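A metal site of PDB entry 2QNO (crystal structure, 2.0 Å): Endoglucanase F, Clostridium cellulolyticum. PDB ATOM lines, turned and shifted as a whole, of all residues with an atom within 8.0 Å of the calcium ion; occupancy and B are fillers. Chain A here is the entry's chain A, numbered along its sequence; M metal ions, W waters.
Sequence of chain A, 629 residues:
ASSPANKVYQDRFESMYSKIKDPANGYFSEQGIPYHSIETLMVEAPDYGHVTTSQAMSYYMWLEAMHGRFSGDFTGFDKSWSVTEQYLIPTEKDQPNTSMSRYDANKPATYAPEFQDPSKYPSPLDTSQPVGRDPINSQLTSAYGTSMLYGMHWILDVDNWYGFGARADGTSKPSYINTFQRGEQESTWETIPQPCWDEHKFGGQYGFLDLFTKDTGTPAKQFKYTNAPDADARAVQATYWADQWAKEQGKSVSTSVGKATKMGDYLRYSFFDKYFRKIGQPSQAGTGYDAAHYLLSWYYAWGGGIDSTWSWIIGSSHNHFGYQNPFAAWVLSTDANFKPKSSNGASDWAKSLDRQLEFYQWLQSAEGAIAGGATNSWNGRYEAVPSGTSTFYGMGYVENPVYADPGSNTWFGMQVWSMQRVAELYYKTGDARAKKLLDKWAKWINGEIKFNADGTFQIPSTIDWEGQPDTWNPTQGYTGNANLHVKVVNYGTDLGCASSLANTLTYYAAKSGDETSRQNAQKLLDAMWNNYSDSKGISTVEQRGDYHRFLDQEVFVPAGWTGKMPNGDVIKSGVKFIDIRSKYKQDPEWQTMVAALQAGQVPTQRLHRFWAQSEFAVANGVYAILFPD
OD2 of Asp 405 is bound to the calcium ion (2.3 Å). The calcium ion is bound by O of Gln 185. The calcium ion is bound by OE2 of Glu 190 (2.4 Å). Water W1 is bound to the calcium ion (2.4 Å). Water W2 is bound to the calcium ion, 2.4 Å away. OE1 of Gln 185 is bound to the calcium ion, 2.6 Å away. OE1 of Glu 190 is bound to the calcium ion (2.6 Å). The calcium ion has seven donor atoms within binding distance.
The side-chain carboxylate (OD1) of Asp 405 lies within salt-bridge range of the guanidinium group (NH1) of Arg 549 (3.0 Å). The side-chain carboxylate of Glu 190 sits close to the guanidinium group of Arg 549, 3.3 Å away. The side-chain carboxylate (OE2) of Glu 190 lies close to the side-chain hydroxyl (OG) of Ser 187 (2.7 Å).
Of the 17 residues printed, 3 come within 4 Å of the calcium ion. The nearest printed residue that does not touch the calcium ion is Arg 549 (4.2 Å).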
ATOM      1  N   GLN A 116       8.395 -10.015  -0.269  1.00  0.00           N
ATOM      2  CA  GLN A 116       9.710 -10.625  -0.070  1.00  0.00           C
ATOM      3  C   GLN A 116      10.761  -9.665   0.506  1.00  0.00           C
ATOM      4  O   GLN A 116      11.915 -10.000   0.592  1.00  0.00           O
ATOM      5  CB  GLN A 116      10.201 -11.257  -1.377  1.00  0.00           C
ATOM      6  CG  GLN A 116       9.529 -12.601  -1.672  1.00  0.00           C
ATOM      7  CD  GLN A 116       8.043 -12.475  -2.006  1.00  0.00           C
ATOM      8  OE1 GLN A 116       7.662 -11.762  -2.934  1.00  0.00           O
ATOM      9  NE2 GLN A 116       7.196 -13.163  -1.244  1.00  0.00           N
ATOM     10  N   ASP A 117      10.365  -8.455   0.876  1.00  0.00           N
ATOM     11  CA  ASP A 117      11.260  -7.541   1.575  1.00  0.00           C
ATOM     12  C   ASP A 117      10.413  -6.806   2.584  1.00  0.00           C
ATOM     13  O   ASP A 117       9.307  -6.370   2.253  1.00  0.00           O
ATOM     14  CB  ASP A 117      11.917  -6.548   0.613  1.00  0.00           C
ATOM     15  CG  ASP A 117      13.038  -5.755   1.281  1.00  0.00           C
ATOM     16  OD1 ASP A 117      14.205  -6.204   1.227  1.00  0.00           O
ATOM     17  OD2 ASP A 117      12.757  -4.709   1.904  1.00  0.00           O
ATOM     18  N   PRO A 118      10.929  -6.675   3.815  1.00  0.00           N
ATOM     19  CA  PRO A 118      10.219  -5.941   4.845  1.00  0.00           C
ATOM     20  C   PRO A 118       9.890  -4.508   4.467  1.00  0.00           C
ATOM     21  O   PRO A 118       8.983  -3.939   5.064  1.00  0.00           O
ATOM     22  CB  PRO A 118      11.219  -5.948   6.026  1.00  0.00           C
ATOM     23  CG  PRO A 118      11.995  -7.204   5.817  1.00  0.00           C
ATOM     24  CD  PRO A 118      12.193  -7.246   4.341  1.00  0.00           C
ATOM     25  N   GLY A 183       7.203 -11.053   6.579  1.00  0.00           N
ATOM     26  CA  GLY A 183       7.554 -11.990   5.499  1.00  0.00           C
ATOM     27  C   GLY A 183       8.920 -12.640   5.559  1.00  0.00           C
ATOM     28  O   GLY A 183       9.607 -12.548   6.575  1.00  0.00           O
ATOM     29  N   GLU A 184       9.315 -13.284   4.458  1.00  0.00           N
ATOM     30  CA  GLU A 184      10.419 -14.259   4.489  1.00  0.00           C
ATOM     31  C   GLU A 184      11.808 -13.649   4.704  1.00  0.00           C
ATOM     32  O   GLU A 184      12.746 -14.362   5.108  1.00  0.00           O
ATOM     33  CB  GLU A 184      10.425 -15.106   3.201  1.00  0.00           C
ATOM     34  CG  GLU A 184      10.790 -14.328   1.957  1.00  0.00           C
ATOM     35  CD  GLU A 184      10.955 -15.218   0.720  1.00  0.00           C
ATOM     36  OE1 GLU A 184      10.275 -16.267   0.639  1.00  0.00           O
ATOM     37  OE2 GLU A 184      11.784 -14.861  -0.144  1.00  0.00           O
ATOM     38  N   GLN A 185      11.954 -12.366   4.419  1.00  0.00           N
ATOM     39  CA  GLN A 185      13.247 -11.731   4.628  1.00  0.00           C
ATOM     40  C   GLN A 185      13.367 -11.007   5.958  1.00  0.00           C
ATOM     41  O   GLN A 185      14.406 -10.426   6.256  1.00  0.00           O
ATOM     42  CB  GLN A 185      13.630 -10.800   3.448  1.00  0.00           C
ATOM     43  CG  GLN A 185      14.532 -11.521   2.406  1.00  0.00           C
ATOM     44  CD  GLN A 185      15.935 -11.842   2.955  1.00  0.00           C
ATOM     45  OE1 GLN A 185      16.436 -11.198   3.898  1.00  0.00           O
ATOM     46  NE2 GLN A 185      16.578 -12.818   2.342  1.00  0.00           N
ATOM     47  N   GLU A 186      12.302 -10.995   6.753  1.00  0.00           N
ATOM     48  CA  GLU A 186      12.380 -10.414   8.078  1.00  0.00           C
ATOM     49  C   GLU A 186      12.980 -11.418   9.072  1.00  0.00           C
ATOM     50  O   GLU A 186      12.241 -12.236   9.620  1.00  0.00           O
ATOM     51  CB  GLU A 186      11.004  -9.984   8.561  1.00  0.00           C
ATOM     52  CG  GLU A 186      11.101  -9.152   9.849  1.00  0.00           C
ATOM     53  CD  GLU A 186       9.741  -8.766  10.396  1.00  0.00           C
ATOM     54  OE1 GLU A 186       8.881  -9.645  10.469  1.00  0.00           O
ATOM     55  OE2 GLU A 186       9.549  -7.588  10.782  1.00  0.00           O
ATOM     56  N   SER A 187      14.287 -11.366   9.298  1.00  0.00           N
ATOM     57  CA  SER A 187      14.926 -12.243  10.284  1.00  0.00           C
ATOM     58  C   SER A 187      14.527 -11.813  11.689  1.00  0.00           C
ATOM     59  O   SER A 187      13.868 -10.793  11.869  1.00  0.00           O
ATOM     60  CB  SER A 187      16.445 -12.166  10.175  1.00  0.00           C
ATOM     61  OG  SER A 187      16.900 -10.882  10.539  1.00  0.00           O
ATOM     62  N   THR A 188      14.980 -12.549  12.691  1.00  0.00           N
ATOM     63  CA  THR A 188      14.746 -12.176  14.084  1.00  0.00           C
ATOM     64  C   THR A 188      15.409 -10.829  14.421  1.00  0.00           C
ATOM     65  O   THR A 188      15.018 -10.153  15.369  1.00  0.00           O
ATOM     66  CB  THR A 188      15.270 -13.292  15.014  1.00  0.00           C
ATOM     67  OG1 THR A 188      14.937 -12.958  16.375  1.00  0.00           O
ATOM     68  CG2 THR A 188      16.705 -13.420  14.896  1.00  0.00           C
ATOM     69  N   TRP A 189      16.402 -10.415  13.608  1.00  0.00           N
ATOM     70  CA  TRP A 189      17.113  -9.161  13.817  1.00  0.00           C
ATOM     71  C   TRP A 189      16.371  -7.919  13.239  1.00  0.00           C
ATOM     72  O   TRP A 189      16.754  -6.767  13.497  1.00  0.00           O
ATOM     73  CB  TRP A 189      18.496  -9.274  13.160  1.00  0.00           C
ATOM     74  CG  TRP A 189      19.313 -10.393  13.722  1.00  0.00           C
ATOM     75  CD1 TRP A 189      19.458 -11.651  13.218  1.00  0.00           C
ATOM     76  CD2 TRP A 189      20.082 -10.343  14.924  1.00  0.00           C
ATOM     77  NE1 TRP A 189      20.315 -12.387  14.019  1.00  0.00           N
ATOM     78  CE2 TRP A 189      20.703 -11.615  15.075  1.00  0.00           C
ATOM     79  CE3 TRP A 189      20.315  -9.352  15.888  1.00  0.00           C
ATOM     80  CZ2 TRP A 189      21.531 -11.919  16.150  1.00  0.00           C
ATOM     81  CZ3 TRP A 189      21.162  -9.648  16.966  1.00  0.00           C
ATOM     82  CH2 TRP A 189      21.761 -10.927  17.076  1.00  0.00           C
ATOM     83  N   GLU A 190      15.321  -8.165  12.465  1.00  0.00           N
ATOM     84  CA  GLU A 190      14.678  -7.127  11.705  1.00  0.00           C
ATOM     85  C   GLU A 190      13.232  -6.817  12.103  1.00  0.00           C
ATOM     86  O   GLU A 190      12.537  -6.081  11.371  1.00  0.00           O
ATOM     87  CB  GLU A 190      14.729  -7.489  10.216  1.00  0.00           C
ATOM     88  CG  GLU A 190      16.136  -7.355   9.632  1.00  0.00           C
ATOM     89  CD  GLU A 190      16.234  -8.091   8.318  1.00  0.00           C
ATOM     90  OE1 GLU A 190      16.101  -7.473   7.238  1.00  0.00           O
ATOM     91  OE2 GLU A 190      16.424  -9.320   8.363  1.00  0.00           O
ATOM     92  N   ALA A 404      13.800 -17.057   4.594  1.00  0.00           N
ATOM     93  CA  ALA A 404      15.040 -17.098   3.793  1.00  0.00           C
ATOM     94  C   ALA A 404      16.239 -16.481   4.519  1.00  0.00           C
ATOM     95  O   ALA A 404      17.342 -16.515   3.994  1.00  0.00           O
ATOM     96  CB  ALA A 404      14.806 -16.363   2.409  1.00  0.00           C
ATOM     97  N   ASP A 405      16.036 -15.898   5.714  1.00  0.00           N
ATOM     98  CA  ASP A 405      17.099 -15.196   6.471  1.00  0.00           C
ATOM     99  C   ASP A 405      17.181 -15.684   7.936  1.00  0.00           C
ATOM    100  O   ASP A 405      16.622 -15.030   8.836  1.00  0.00           O
ATOM    101  CB  ASP A 405      16.821 -13.679   6.430  1.00  0.00           C
ATOM    102  CG  ASP A 405      17.971 -12.802   6.930  1.00  0.00           C
ATOM    103  OD1 ASP A 405      19.001 -13.297   7.453  1.00  0.00           O
ATOM    104  OD2 ASP A 405      17.798 -11.549   6.800  1.00  0.00           O
ATOM    105  N   PRO A 406      17.858 -16.813   8.203  1.00  0.00           N
ATOM    106  CA  PRO A 406      18.484 -17.738   7.264  1.00  0.00           C
ATOM    107  C   PRO A 406      17.419 -18.694   6.693  1.00  0.00           C
ATOM    108  O   PRO A 406      16.278 -18.721   7.201  1.00  0.00           O
ATOM    109  CB  PRO A 406      19.473 -18.496   8.160  1.00  0.00           C
ATOM    110  CG  PRO A 406      18.821 -18.537   9.499  1.00  0.00           C
ATOM    111  CD  PRO A 406      18.028 -17.249   9.609  1.00  0.00           C
ATOM    112  N   ARG A 549      24.951  -8.412  14.120  1.00  0.00           N
ATOM    113  CA  ARG A 549      23.676  -7.781  13.769  1.00  0.00           C
ATOM    114  C   ARG A 549      23.043  -6.952  14.901  1.00  0.00           C
ATOM    115  O   ARG A 549      22.200  -6.089  14.614  1.00  0.00           O
ATOM    116  CB  ARG A 549      22.700  -8.821  13.186  1.00  0.00           C
ATOM    117  CG  ARG A 549      23.281  -9.430  11.874  1.00  0.00           C
ATOM    118  CD  ARG A 549      22.431 -10.546  11.294  1.00  0.00           C
ATOM    119  NE  ARG A 549      21.337  -9.990  10.508  1.00  0.00           N
ATOM    120  CZ  ARG A 549      20.526 -10.684   9.715  1.00  0.00           C
ATOM    121  NH1 ARG A 549      20.652 -12.013   9.602  1.00  0.00           N
ATOM    122  NH2 ARG A 549      19.590 -10.050   9.034  1.00  0.00           N
ATOM    123  N   GLN A 553      22.516  -4.161  12.195  1.00  0.00           N
ATOM    124  CA  GLN A 553      21.295  -4.474  11.427  1.00  0.00           C
ATOM    125  C   GLN A 553      20.338  -3.298  11.483  1.00  0.00           C
ATOM    126  O   GLN A 553      19.829  -2.965  12.548  1.00  0.00           O
ATOM    127  CB  GLN A 553      20.594  -5.740  11.930  1.00  0.00           C
ATOM    128  CG  GLN A 553      19.303  -6.075  11.179  1.00  0.00           C
ATOM    129  CD  GLN A 553      19.572  -6.435   9.741  1.00  0.00           C
ATOM    130  OE1 GLN A 553      20.291  -7.389   9.453  1.00  0.00           O
ATOM    131  NE2 GLN A 553      19.007  -5.667   8.815  1.00  0.00           N
ATOM    132  N   GLU A 554      20.083  -2.672  10.334  1.00  0.00           N
ATOM    133  CA  GLU A 554      19.060  -1.624  10.299  1.00  0.00           C
ATOM    134  C   GLU A 554      17.673  -2.265  10.326  1.00  0.00           C
ATOM    135  O   GLU A 554      17.450  -3.259   9.676  1.00  0.00           O
ATOM    136  CB  GLU A 554      19.185  -0.751   9.043  1.00  0.00           C
ATOM    137  CG  GLU A 554      18.101   0.343   8.949  1.00  0.00           C
ATOM    138  CD  GLU A 554      18.262   1.273   7.732  1.00  0.00           C
ATOM    139  OE1 GLU A 554      19.426   1.615   7.401  1.00  0.00           O
ATOM    140  OE2 GLU A 554      17.210   1.641   7.114  1.00  0.00           O
HETATM  141 CA    CA M   1      16.610  -9.730   6.022  1.00  0.00          CA
HETATM  142  O   HOH W   1      15.900  -8.104   4.430  1.00  0.00           O
HETATM  143  O   HOH W   2      18.878  -8.939   5.715  1.00  0.00           O
